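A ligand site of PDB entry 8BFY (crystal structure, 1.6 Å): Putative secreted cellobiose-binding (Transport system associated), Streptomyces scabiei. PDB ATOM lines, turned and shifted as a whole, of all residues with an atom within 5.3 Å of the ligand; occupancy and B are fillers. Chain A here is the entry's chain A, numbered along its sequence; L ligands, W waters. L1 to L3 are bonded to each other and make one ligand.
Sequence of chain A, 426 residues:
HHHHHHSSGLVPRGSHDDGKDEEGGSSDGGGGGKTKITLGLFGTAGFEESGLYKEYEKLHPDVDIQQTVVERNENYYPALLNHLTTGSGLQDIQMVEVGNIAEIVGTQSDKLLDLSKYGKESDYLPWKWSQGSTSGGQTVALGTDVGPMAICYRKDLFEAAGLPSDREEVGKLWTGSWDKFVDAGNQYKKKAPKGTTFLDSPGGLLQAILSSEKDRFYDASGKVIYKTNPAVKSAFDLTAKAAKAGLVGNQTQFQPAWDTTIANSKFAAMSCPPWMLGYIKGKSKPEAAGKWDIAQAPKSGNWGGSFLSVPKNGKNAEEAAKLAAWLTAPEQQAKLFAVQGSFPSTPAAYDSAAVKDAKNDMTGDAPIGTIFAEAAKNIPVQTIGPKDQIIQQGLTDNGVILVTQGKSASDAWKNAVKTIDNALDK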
ATOM      1  N   PHE A  42      19.620 -26.297 -18.843  1.00  0.00           N
ATOM      2  CA  PHE A  42      20.146 -25.785 -20.108  1.00  0.00           C
ATOM      3  C   PHE A  42      19.029 -25.074 -20.852  1.00  0.00           C
ATOM      4  O   PHE A  42      17.870 -25.165 -20.475  1.00  0.00           O
ATOM      5  CB  PHE A  42      20.777 -26.896 -20.949  1.00  0.00           C
ATOM      6  CG  PHE A  42      19.818 -27.978 -21.355  1.00  0.00           C
ATOM      7  CD1 PHE A  42      18.996 -27.811 -22.466  1.00  0.00           C
ATOM      8  CD2 PHE A  42      19.714 -29.140 -20.603  1.00  0.00           C
ATOM      9  CE1 PHE A  42      18.115 -28.812 -22.822  1.00  0.00           C
ATOM     10  CE2 PHE A  42      18.820 -30.124 -20.950  1.00  0.00           C
ATOM     11  CZ  PHE A  42      17.997 -29.952 -22.039  1.00  0.00           C
ATOM     12  N   GLY A  43      19.414 -24.376 -21.919  1.00  0.00           N
ATOM     13  CA  GLY A  43      18.412 -23.762 -22.780  1.00  0.00           C
ATOM     14  C   GLY A  43      17.560 -22.760 -22.020  1.00  0.00           C
ATOM     15  O   GLY A  43      18.055 -22.031 -21.177  1.00  0.00           O
ATOM     16  N   THR A  44      16.259 -22.761 -22.358  1.00  0.00           N
ATOM     17  CA  THR A  44      15.267 -21.906 -21.723  1.00  0.00           C
ATOM     18  C   THR A  44      14.121 -22.795 -21.231  1.00  0.00           C
ATOM     19  O   THR A  44      13.081 -22.939 -21.890  1.00  0.00           O
ATOM     20  CB  THR A  44      14.779 -20.822 -22.696  1.00  0.00           C
ATOM     21  OG1 THR A  44      15.904 -20.125 -23.250  1.00  0.00           O
ATOM     22  CG2 THR A  44      13.854 -19.827 -22.048  1.00  0.00           C
ATOM     23  N   ALA A  45      14.315 -23.396 -20.061  1.00  0.00           N
ATOM     24  CA  ALA A  45      13.343 -24.331 -19.528  1.00  0.00           C
ATOM     25  C   ALA A  45      11.985 -23.665 -19.325  1.00  0.00           C
ATOM     26  O   ALA A  45      10.958 -24.294 -19.560  1.00  0.00           O
ATOM     27  CB  ALA A  45      13.861 -24.931 -18.250  1.00  0.00           C
ATOM     28  N   GLU A  71      23.719 -22.424 -21.445  1.00  0.00           N
ATOM     29  CA  GLU A  71      22.853 -22.119 -22.569  1.00  0.00           C
ATOM     30  C   GLU A  71      22.676 -23.294 -23.520  1.00  0.00           C
ATOM     31  O   GLU A  71      21.554 -23.645 -23.868  1.00  0.00           O
ATOM     32  CB  GLU A  71      23.412 -20.889 -23.286  1.00  0.00           C
ATOM     33  CG  GLU A  71      23.579 -19.674 -22.385  1.00  0.00           C
ATOM     34  CD  GLU A  71      24.520 -18.599 -22.926  1.00  0.00           C
ATOM     35  OE1 GLU A  71      25.778 -18.777 -22.866  1.00  0.00           O
ATOM     36  OE2 GLU A  71      23.992 -17.584 -23.400  1.00  0.00           O
ATOM     37  N   ARG A  72      23.771 -23.904 -23.983  1.00  0.00           N
ATOM     38  CA  ARG A  72      23.697 -24.946 -24.995  1.00  0.00           C
ATOM     39  C   ARG A  72      23.830 -26.328 -24.361  1.00  0.00           C
ATOM     40  O   ARG A  72      24.743 -26.566 -23.584  1.00  0.00           O
ATOM     41  CB  ARG A  72      24.822 -24.773 -26.031  1.00  0.00           C
ATOM     42  CG  ARG A  72      24.713 -23.514 -26.881  1.00  0.00           C
ATOM     43  CD  ARG A  72      25.968 -23.209 -27.670  1.00  0.00           C
ATOM     44  NE  ARG A  72      26.362 -24.286 -28.542  1.00  0.00           N
ATOM     45  CZ  ARG A  72      25.830 -24.558 -29.726  1.00  0.00           C
ATOM     46  NH1 ARG A  72      24.824 -23.845 -30.187  1.00  0.00           N
ATOM     47  NH2 ARG A  72      26.327 -25.522 -30.481  1.00  0.00           N
ATOM     48  N   ASN A  73      22.958 -27.261 -24.745  1.00  0.00           N
ATOM     49  CA  ASN A  73      23.035 -28.627 -24.277  1.00  0.00           C
ATOM     50  C   ASN A  73      24.389 -29.235 -24.621  1.00  0.00           C
ATOM     51  O   ASN A  73      24.924 -30.023 -23.828  1.00  0.00           O
ATOM     52  CB  ASN A  73      21.858 -29.460 -24.799  1.00  0.00           C
ATOM     53  CG  ASN A  73      21.793 -30.808 -24.130  1.00  0.00           C
ATOM     54  OD1 ASN A  73      21.926 -30.907 -22.895  1.00  0.00           O
ATOM     55  ND2 ASN A  73      21.546 -31.833 -24.918  1.00  0.00           N
ATOM     56  N   GLU A  74      24.976 -28.841 -25.757  1.00  0.00           N
ATOM     57  CA  GLU A  74      26.307 -29.310 -26.150  1.00  0.00           C
ATOM     58  C   GLU A  74      27.315 -29.146 -25.007  1.00  0.00           C
ATOM     59  O   GLU A  74      28.164 -30.006 -24.836  1.00  0.00           O
ATOM     60  CB  GLU A  74      26.813 -28.511 -27.363  1.00  0.00           C
ATOM     61  CG  GLU A  74      28.265 -28.786 -27.682  1.00  0.00           C
ATOM     62  CD  GLU A  74      28.736 -28.247 -29.015  1.00  0.00           C
ATOM     63  OE1 GLU A  74      27.909 -27.804 -29.814  1.00  0.00           O
ATOM     64  OE2 GLU A  74      29.941 -28.307 -29.253  1.00  0.00           O
ATOM     65  N   MET A  95      18.440 -31.095 -15.230  1.00  0.00           N
ATOM     66  CA  MET A  95      17.642 -31.318 -16.430  1.00  0.00           C
ATOM     67  C   MET A  95      18.375 -32.277 -17.383  1.00  0.00           C
ATOM     68  O   MET A  95      19.610 -32.336 -17.386  1.00  0.00           O
ATOM     69  CB  MET A  95      17.455 -29.938 -17.061  1.00  0.00           C
ATOM     70  CG  MET A  95      16.494 -29.832 -18.229  1.00  0.00           C
ATOM     71  SD  MET A  95      16.394 -28.060 -18.679  1.00  0.00           S
ATOM     72  CE  MET A  95      15.418 -28.194 -20.180  1.00  0.00           C
ATOM     73  N   GLU A  97      18.004 -33.722 -21.550  1.00  0.00           N
ATOM     74  CA  GLU A  97      17.334 -33.724 -22.853  1.00  0.00           C
ATOM     75  C   GLU A  97      17.078 -35.154 -23.317  1.00  0.00           C
ATOM     76  O   GLU A  97      17.849 -36.069 -23.033  1.00  0.00           O
ATOM     77  CB  GLU A  97      18.095 -32.898 -23.901  1.00  0.00           C
ATOM     78  CG  GLU A  97      17.185 -32.163 -24.935  1.00  0.00           C
ATOM     79  CD  GLU A  97      17.094 -32.777 -26.317  1.00  0.00           C
ATOM     80  OE1 GLU A  97      17.865 -33.764 -26.622  1.00  0.00           O
ATOM     81  OE2 GLU A  97      16.288 -32.238 -27.104  1.00  0.00           O
ATOM     82  N   VAL A  98      16.045 -35.350 -24.144  1.00  0.00           N
ATOM     83  CA  VAL A  98      15.702 -36.664 -24.682  1.00  0.00           C
ATOM     84  C   VAL A  98      16.859 -37.259 -25.517  1.00  0.00           C
ATOM     85  O   VAL A  98      16.968 -38.491 -25.635  1.00  0.00           O
ATOM     86  CB  VAL A  98      14.382 -36.611 -25.477  1.00  0.00           C
ATOM     87  CG1 VAL A  98      14.460 -35.765 -26.739  1.00  0.00           C
ATOM     88  CG2 VAL A  98      13.892 -38.035 -25.773  1.00  0.00           C
ATOM     89  N   THR A 144       9.370 -33.302 -18.607  1.00  0.00           N
ATOM     90  CA  THR A 144       8.897 -31.937 -18.770  1.00  0.00           C
ATOM     91  C   THR A 144       7.985 -31.917 -19.999  1.00  0.00           C
ATOM     92  O   THR A 144       6.834 -32.382 -19.949  1.00  0.00           O
ATOM     93  CB  THR A 144      10.057 -30.944 -18.749  1.00  0.00           C
ATOM     94  OG1 THR A 144      10.942 -31.136 -19.863  1.00  0.00           O
ATOM     95  CG2 THR A 144      10.831 -30.974 -17.450  1.00  0.00           C
ATOM     96  N   ASP A 145       8.507 -31.405 -21.127  1.00  0.00           N
ATOM     97  CA  ASP A 145       7.732 -31.134 -22.322  1.00  0.00           C
ATOM     98  C   ASP A 145       7.937 -32.208 -23.385  1.00  0.00           C
ATOM     99  O   ASP A 145       8.755 -33.120 -23.255  1.00  0.00           O
ATOM    100  CB  ASP A 145       8.069 -29.740 -22.840  1.00  0.00           C
ATOM    101  CG  ASP A 145       9.485 -29.512 -23.332  1.00  0.00           C
ATOM    102  OD1 ASP A 145      10.410 -30.323 -22.968  1.00  0.00           O
ATOM    103  OD2 ASP A 145       9.675 -28.552 -24.079  1.00  0.00           O
ATOM    104  N   GLN A 207      16.423 -30.620 -38.669  1.00  0.00           N
ATOM    105  CA  GLN A 207      15.767 -31.155 -37.473  1.00  0.00           C
ATOM    106  C   GLN A 207      14.272 -31.335 -37.735  1.00  0.00           C
ATOM    107  O   GLN A 207      13.679 -32.323 -37.309  1.00  0.00           O
ATOM    108  CB  GLN A 207      16.044 -30.235 -36.286  1.00  0.00           C
ATOM    109  CG  GLN A 207      17.506 -30.241 -35.820  1.00  0.00           C
ATOM    110  CD  GLN A 207      17.845 -31.286 -34.784  1.00  0.00           C
ATOM    111  OE1 GLN A 207      17.250 -32.361 -34.683  1.00  0.00           O
ATOM    112  NE2 GLN A 207      18.798 -30.939 -33.937  1.00  0.00           N
ATOM    113  N   GLN A 253      22.352 -22.752 -35.088  1.00  0.00           N
ATOM    114  CA  GLN A 253      21.313 -22.388 -34.135  1.00  0.00           C
ATOM    115  C   GLN A 253      21.893 -22.292 -32.719  1.00  0.00           C
ATOM    116  O   GLN A 253      22.920 -22.889 -32.424  1.00  0.00           O
ATOM    117  CB  GLN A 253      20.165 -23.395 -34.143  1.00  0.00           C
ATOM    118  CG  GLN A 253      19.397 -23.457 -35.446  1.00  0.00           C
ATOM    119  CD  GLN A 253      18.160 -24.303 -35.286  1.00  0.00           C
ATOM    120  OE1 GLN A 253      18.229 -25.488 -34.971  1.00  0.00           O
ATOM    121  NE2 GLN A 253      16.989 -23.698 -35.478  1.00  0.00           N
ATOM    122  N   PHE A 254      21.199 -21.539 -31.863  1.00  0.00           N
ATOM    123  CA  PHE A 254      21.478 -21.447 -30.430  1.00  0.00           C
ATOM    124  C   PHE A 254      22.875 -20.879 -30.168  1.00  0.00           C
ATOM    125  O   PHE A 254      23.569 -21.344 -29.246  1.00  0.00           O
ATOM    126  CB  PHE A 254      21.250 -22.809 -29.765  1.00  0.00           C
ATOM    127  CG  PHE A 254      19.926 -23.420 -30.107  1.00  0.00           C
ATOM    128  CD1 PHE A 254      18.745 -22.799 -29.745  1.00  0.00           C
ATOM    129  CD2 PHE A 254      19.839 -24.513 -30.938  1.00  0.00           C
ATOM    130  CE1 PHE A 254      17.531 -23.348 -30.082  1.00  0.00           C
ATOM    131  CE2 PHE A 254      18.616 -25.062 -31.290  1.00  0.00           C
ATOM    132  CZ  PHE A 254      17.453 -24.451 -30.870  1.00  0.00           C
ATOM    133  N   TRP A 275       8.653 -25.513 -27.580  1.00  0.00           N
ATOM    134  CA  TRP A 275       9.700 -24.907 -26.777  1.00  0.00           C
ATOM    135  C   TRP A 275      10.530 -23.870 -27.542  1.00  0.00           C
ATOM    136  O   TRP A 275      11.214 -23.044 -26.951  1.00  0.00           O
ATOM    137  CB  TRP A 275      10.613 -25.985 -26.173  1.00  0.00           C
ATOM    138  CG  TRP A 275      11.258 -26.919 -27.161  1.00  0.00           C
ATOM    139  CD1 TRP A 275      10.819 -28.171 -27.497  1.00  0.00           C
ATOM    140  CD2 TRP A 275      12.452 -26.695 -27.964  1.00  0.00           C
ATOM    141  NE1 TRP A 275      11.631 -28.727 -28.441  1.00  0.00           N
ATOM    142  CE2 TRP A 275      12.647 -27.854 -28.734  1.00  0.00           C
ATOM    143  CE3 TRP A 275      13.376 -25.647 -28.087  1.00  0.00           C
ATOM    144  CZ2 TRP A 275      13.717 -27.981 -29.626  1.00  0.00           C
ATOM    145  CZ3 TRP A 275      14.427 -25.764 -28.973  1.00  0.00           C
ATOM    146  CH2 TRP A 275      14.601 -26.914 -29.728  1.00  0.00           C
ATOM    147  N   TYR A 279      12.703 -19.383 -27.033  1.00  0.00           N
ATOM    148  CA  TYR A 279      13.784 -18.699 -27.732  1.00  0.00           C
ATOM    149  C   TYR A 279      13.282 -17.496 -28.497  1.00  0.00           C
ATOM    150  O   TYR A 279      13.918 -16.445 -28.450  1.00  0.00           O
ATOM    151  CB  TYR A 279      14.523 -19.675 -28.653  1.00  0.00           C
ATOM    152  CG  TYR A 279      15.387 -20.667 -27.923  1.00  0.00           C
ATOM    153  CD1 TYR A 279      16.636 -20.285 -27.452  1.00  0.00           C
ATOM    154  CD2 TYR A 279      14.943 -21.950 -27.657  1.00  0.00           C
ATOM    155  CE1 TYR A 279      17.450 -21.177 -26.787  1.00  0.00           C
ATOM    156  CE2 TYR A 279      15.753 -22.859 -26.974  1.00  0.00           C
ATOM    157  CZ  TYR A 279      16.990 -22.448 -26.524  1.00  0.00           C
ATOM    158  OH  TYR A 279      17.818 -23.364 -25.890  1.00  0.00           O
ATOM    159  N   TRP A 303      10.421 -33.000 -32.180  1.00  0.00           N
ATOM    160  CA  TRP A 303      11.785 -32.560 -31.928  1.00  0.00           C
ATOM    161  C   TRP A 303      11.879 -32.060 -30.489  1.00  0.00           C
ATOM    162  O   TRP A 303      11.363 -31.002 -30.162  1.00  0.00           O
ATOM    163  CB  TRP A 303      12.283 -31.518 -32.932  1.00  0.00           C
ATOM    164  CG  TRP A 303      13.640 -30.961 -32.641  1.00  0.00           C
ATOM    165  CD1 TRP A 303      14.644 -31.564 -31.938  1.00  0.00           C
ATOM    166  CD2 TRP A 303      14.194 -29.702 -33.098  1.00  0.00           C
ATOM    167  NE1 TRP A 303      15.742 -30.758 -31.884  1.00  0.00           N
ATOM    168  CE2 TRP A 303      15.514 -29.616 -32.590  1.00  0.00           C
ATOM    169  CE3 TRP A 303      13.710 -28.641 -33.860  1.00  0.00           C
ATOM    170  CZ2 TRP A 303      16.338 -28.509 -32.812  1.00  0.00           C
ATOM    171  CZ3 TRP A 303      14.522 -27.546 -34.067  1.00  0.00           C
ATOM    172  CH2 TRP A 303      15.827 -27.487 -33.590  1.00  0.00           C
ATOM    173  N   GLY A 304      12.597 -32.815 -29.650  1.00  0.00           N
ATOM    174  CA  GLY A 304      12.935 -32.421 -28.307  1.00  0.00           C
ATOM    175  C   GLY A 304      12.010 -33.024 -27.244  1.00  0.00           C
ATOM    176  O   GLY A 304      11.210 -33.928 -27.504  1.00  0.00           O
ATOM    177  N   GLY A 305      12.150 -32.460 -26.046  1.00  0.00           N
ATOM    178  CA  GLY A 305      11.561 -33.000 -24.828  1.00  0.00           C
ATOM    179  C   GLY A 305      12.647 -33.243 -23.791  1.00  0.00           C
ATOM    180  O   GLY A 305      13.776 -33.585 -24.155  1.00  0.00           O
ATOM    181  N   SER A 306      12.320 -32.970 -22.531  1.00  0.00           N
ATOM    182  CA  SER A 306      13.310 -33.032 -21.463  1.00  0.00           C
ATOM    183  C   SER A 306      12.712 -33.692 -20.215  1.00  0.00           C
ATOM    184  O   SER A 306      11.555 -34.140 -20.197  1.00  0.00           O
ATOM    185  CB  SER A 306      13.884 -31.665 -21.170  1.00  0.00           C
ATOM    186  OG  SER A 306      14.607 -31.156 -22.284  1.00  0.00           O
ATOM    187  N   SER A 342       5.991 -24.130 -24.030  1.00  0.00           N
ATOM    188  CA  SER A 342       6.414 -25.516 -24.079  1.00  0.00           C
ATOM    189  C   SER A 342       5.251 -26.455 -23.750  1.00  0.00           C
ATOM    190  O   SER A 342       4.487 -26.216 -22.801  1.00  0.00           O
ATOM    191  CB  SER A 342       7.564 -25.757 -23.159  1.00  0.00           C
ATOM    192  OG  SER A 342       8.672 -24.923 -23.482  1.00  0.00           O
ATOM    193  N   GLN A 389      21.896 -37.177 -29.192  1.00  0.00           N
ATOM    194  CA  GLN A 389      22.315 -35.794 -29.087  1.00  0.00           C
ATOM    195  C   GLN A 389      23.548 -35.521 -29.953  1.00  0.00           C
ATOM    196  O   GLN A 389      23.595 -34.518 -30.654  1.00  0.00           O
ATOM    197  CB  GLN A 389      22.502 -35.382 -27.621  1.00  0.00           C
ATOM    198  CG  GLN A 389      23.155 -34.021 -27.419  1.00  0.00           C
ATOM    199  CD  GLN A 389      24.633 -34.064 -27.114  1.00  0.00           C
ATOM    200  OE1 GLN A 389      25.121 -34.988 -26.477  1.00  0.00           O
ATOM    201  NE2 GLN A 389      25.352 -33.033 -27.544  1.00  0.00           N
ATOM    202  N   GLN A 392      22.751 -35.726 -33.734  1.00  0.00           N
ATOM    203  CA  GLN A 392      22.079 -34.498 -34.136  1.00  0.00           C
ATOM    204  C   GLN A 392      23.080 -33.366 -34.315  1.00  0.00           C
ATOM    205  O   GLN A 392      23.013 -32.579 -35.273  1.00  0.00           O
ATOM    206  CB  GLN A 392      21.031 -34.088 -33.092  1.00  0.00           C
ATOM    207  CG  GLN A 392      19.723 -34.891 -33.173  1.00  0.00           C
ATOM    208  CD  GLN A 392      18.860 -34.647 -31.968  1.00  0.00           C
ATOM    209  OE1 GLN A 392      19.159 -35.078 -30.863  1.00  0.00           O
ATOM    210  NE2 GLN A 392      17.794 -33.903 -32.145  1.00  0.00           N
ATOM    211  N   GLN A 393      24.026 -33.269 -33.375  1.00  0.00           N
ATOM    212  CA  GLN A 393      24.963 -32.175 -33.380  1.00  0.00           C
ATOM    213  C   GLN A 393      25.860 -32.266 -34.612  1.00  0.00           C
ATOM    214  O   GLN A 393      26.173 -31.252 -35.255  1.00  0.00           O
ATOM    215  CB  GLN A 393      25.753 -32.182 -32.071  1.00  0.00           C
ATOM    216  CG  GLN A 393      26.797 -31.082 -31.954  1.00  0.00           C
ATOM    217  CD  GLN A 393      27.494 -31.137 -30.620  1.00  0.00           C
ATOM    218  OE1 GLN A 393      26.870 -31.038 -29.563  1.00  0.00           O
ATOM    219  NE2 GLN A 393      28.796 -31.368 -30.662  1.00  0.00           N
ATOM    220  N   THR A 396      24.071 -31.360 -37.981  1.00  0.00           N
ATOM    221  CA  THR A 396      23.742 -29.951 -38.121  1.00  0.00           C
ATOM    222  C   THR A 396      25.023 -29.122 -38.184  1.00  0.00           C
ATOM    223  O   THR A 396      25.375 -28.583 -39.246  1.00  0.00           O
ATOM    224  CB  THR A 396      22.737 -29.509 -37.037  1.00  0.00           C
ATOM    225  OG1 THR A 396      23.248 -29.760 -35.723  1.00  0.00           O
ATOM    226  CG2 THR A 396      21.389 -30.201 -37.197  1.00  0.00           C
ATOM    227  N   ASP A 397      25.733 -29.015 -37.053  1.00  0.00           N
ATOM    228  CA  ASP A 397      26.860 -28.124 -36.879  1.00  0.00           C
ATOM    229  C   ASP A 397      28.127 -28.611 -37.596  1.00  0.00           C
ATOM    230  O   ASP A 397      29.046 -27.823 -37.797  1.00  0.00           O
ATOM    231  CB  ASP A 397      27.130 -27.880 -35.392  1.00  0.00           C
ATOM    232  CG  ASP A 397      26.063 -27.078 -34.653  1.00  0.00           C
ATOM    233  OD1 ASP A 397      25.107 -26.596 -35.296  1.00  0.00           O
ATOM    234  OD2 ASP A 397      26.213 -26.942 -33.427  1.00  0.00           O
HETATM  235  C1  LIG L   1      21.962 -28.836 -32.378  1.00  0.00           C
HETATM  236  C2  LIG L   1      20.970 -28.061 -31.543  1.00  0.00           C
HETATM  237  C3  LIG L   1      21.509 -27.886 -30.127  1.00  0.00           C
HETATM  238  C4  LIG L   1      22.903 -27.260 -30.133  1.00  0.00           C
HETATM  239  C5  LIG L   1      23.496 -27.122 -28.748  1.00  0.00           C
HETATM  240  C6  LIG L   1      23.329 -28.174 -32.301  1.00  0.00           C
HETATM  241  O1  LIG L   1      24.274 -28.872 -32.990  1.00  0.00           O
HETATM  242  O2  LIG L   1      21.488 -28.938 -33.706  1.00  0.00           O
HETATM  243  O3  LIG L   1      19.723 -28.767 -31.555  1.00  0.00           O
HETATM  244  O4  LIG L   1      20.637 -27.039 -29.358  1.00  0.00           O
HETATM  245  O5  LIG L   1      23.776 -28.071 -30.961  1.00  0.00           O
HETATM  246  O6  LIG L   1      23.390 -28.315 -27.981  1.00  0.00           O
HETATM  247  C1  LG2 L   2      19.462 -26.646 -27.313  1.00  0.00           C
HETATM  248  C2  LG2 L   2      18.386 -27.181 -26.385  1.00  0.00           C
HETATM  249  C3  LG2 L   2      17.351 -27.992 -27.145  1.00  0.00           C
HETATM  250  C4  LG2 L   2      17.964 -28.982 -28.132  1.00  0.00           C
HETATM  251  C5  LG2 L   2      16.943 -29.715 -28.980  1.00  0.00           C
HETATM  252  C6  LG2 L   2      19.939 -27.686 -28.322  1.00  0.00           C
HETATM  253  O1  LG2 L   2      20.566 -26.172 -26.534  1.00  0.00           O
HETATM  254  O2  LG2 L   2      17.779 -26.088 -25.667  1.00  0.00           O
HETATM  255  O3  LG2 L   2      16.602 -28.776 -26.256  1.00  0.00           O
HETATM  256  O4  LG2 L   2      18.836 -28.285 -29.015  1.00  0.00           O
HETATM  257  O5  LG2 L   2      17.545 -30.841 -29.609  1.00  0.00           O
HETATM  258  C1  LG3 L   3      14.595 -29.518 -25.311  1.00  0.00           C
HETATM  259  C2  LG3 L   3      13.264 -29.148 -24.668  1.00  0.00           C
HETATM  260  C3  LG3 L   3      13.406 -27.966 -23.706  1.00  0.00           C
HETATM  261  C4  LG3 L   3      14.161 -26.812 -24.413  1.00  0.00           C
HETATM  262  C5  LG3 L   3      14.455 -25.632 -23.518  1.00  0.00           C
HETATM  263  C6  LG3 L   3      15.315 -28.340 -25.887  1.00  0.00           C
HETATM  264  O1  LG3 L   3      14.339 -30.507 -26.300  1.00  0.00           O
HETATM  265  O2  LG3 L   3      12.766 -30.297 -24.003  1.00  0.00           O
HETATM  266  O3  LG3 L   3      12.129 -27.555 -23.231  1.00  0.00           O
HETATM  267  O4  LG3 L   3      15.438 -27.323 -24.895  1.00  0.00           O
HETATM  268  O5  LG3 L   3      15.077 -24.530 -24.214  1.00  0.00           O
HETATM  269  O   HOH W   1      16.094 -33.728 -29.608  1.00  0.00           O
HETATM  270  O   HOH W   2      24.364 -30.659 -28.958  1.00  0.00           O
HETATM  271  O   HOH W   3      20.576 -23.461 -26.352  1.00  0.00           O
HETATM  272  O   HOH W   4      19.897 -31.548 -31.207  1.00  0.00           O
HETATM  273  O   HOH W   5      19.277 -33.302 -28.784  1.00  0.00           O
HETATM  274  O   HOH W   6      20.466 -26.965 -35.402  1.00  0.00           O
HETATM  275  O   HOH W   7      12.726 -23.241 -24.750  1.00  0.00           O
HETATM  276  O   HOH W   8      10.825 -25.296 -22.207  1.00  0.00           O
HETATM  277  O   HOH W   9      11.907 -28.585 -20.457  1.00  0.00           O
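Residues that only touch the ligand: Phe 42 (3.7 Å), Gly 43 (3.7 Å), Glu 71 (3.8 Å), Arg 72 (3.6 Å), Phe 254 (3.1 Å), Trp 275 (3.7 Å), Gly 304 (3.1 Å), Gln 392 (3.98 Å) and Gln 393 (3.4 Å). The nearest printed residue that does not touch the ligand is Met 95 (4.1 Å).
The guanidinium group (NH2) of Arg 72 lies within salt-bridge range of the side-chain carboxylate (OD2) of Asp 397, at 3.3 Å. OE1 of Glu 74 is in salt-bridge range of NH2 of Arg 72 (2.9 Å). The backbone carbonyl oxygen of Gln 392 lies within hydrogen-bond range of the side-chain hydroxyl of Thr 396 (2.9 Å). The backbone carbonyl oxygen (O) of Phe 254 is in hydrogen-bond range of the guanidinium group (NH1) of Arg 72 (3.0 Å). NE2 of Gln 392 is in hydrogen-bond range of OE1 of Gln 207 (3.0 Å). The side-chain amide oxygen (OE1) of Gln 393 is in hydrogen-bond range of the side-chain amide nitrogen (NE2) of Gln 389. The backbone NH of Phe 42 is in hydrogen-bond range of the side-chain sulfur of Met 95 (3.7 Å). N of Gly 43 lies within hydrogen-bond range of O of Glu 71 (3.0 Å).
The side-chain carboxylate (OD1) of Asp 145 is in hydrogen-bond range of an oxygen (O2) of LG3 L3, 2.6 Å away. N of Ser 306 sits at hydrogen-bond distance from O2 of LG3 L3 (3.1 Å). O2 of LG3 L3 is in hydrogen-bond range of OG of Ser 306 (2.7 Å). OE2 of Glu 97 lies within hydrogen-bond range of O1 of LG3 L3 (2.7 Å). An oxygen (O2) of LG2 L2 is in hydrogen-bond range of the side-chain hydroxyl (OH) of Tyr 279 (2.7 Å). The side-chain carboxylate (OD2) of Asp 397 is in hydrogen-bond range of an oxygen (O1) of LIG L1 (2.8 Å). An oxygen (O6) of LIG L1 sits at hydrogen-bond distance from the backbone NH of Glu 74 (2.8 Å). O2 of LIG L1 sits at hydrogen-bond distance from OG1 of Thr 396 (2.8 Å). An oxygen (O5) of LG3 L3 lies within hydrogen-bond range of the backbone NH (N) of Thr 44, at 2.8 Å. The backbone carbonyl oxygen (O) of Thr 44 sits close to an oxygen (O5) of LG3 L3. NE1 of Trp 303 sits at hydrogen-bond distance from O5 of LG2 L2 (2.9 Å). The backbone NH (N) of Gly 305 lies within hydrogen-bond range of an oxygen (O1) of LG3 L3. An oxygen (O2) of LG3 L3 lies close to the backbone carbonyl oxygen (O) of Gly 305 (3.4 Å). N of Asn 73 lies within hydrogen-bond range of O1 of LG2 L2 (3.2 Å). O3 of LIG L1 sits at hydrogen-bond distance from NE2 of Gln 207 (3.4 Å).
Water W3 lies within hydrogen-bond range of the backbone carbonyl oxygen (O) of Glu 71 (2.7 Å), an oxygen (O1) of LG2 L2 (2.7 Å) and the side-chain hydroxyl (OH) of Tyr 279 (2.8 Å). Water W2 lies within hydrogen-bond range of OE1 of Gln 393 (2.6 Å), O6 of LIG L1 (2.7 Å) and NE2 of Gln 389 (2.9 Å). Water W8 lies within hydrogen-bond range of the side-chain hydroxyl of Ser 342 (2.5 Å), an oxygen (O3) of LG3 L3 (2.8 Å), the backbone carbonyl oxygen of Ala 45 (2.8 Å) and the backbone carbonyl oxygen of Thr 44 (3.3 Å). Water W4 lies within hydrogen-bond range of O3 of LIG L1 (2.8 Å), NE2 of Gln 207 (3.0 Å) and NE2 of Gln 392 (3.3 Å). Water W9 lies within hydrogen-bond range of OG1 of Thr 144 (2.8 Å), O3 of LG3 L3 (3.0 Å) and OD1 of Asp 145 (3.4 Å). Water W5 lies within hydrogen-bond range of the side-chain carboxylate (OE1) of Glu 97, the side-chain amide oxygen (OE1) of Gln 392 and an oxygen (O5) of LG2 L2.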
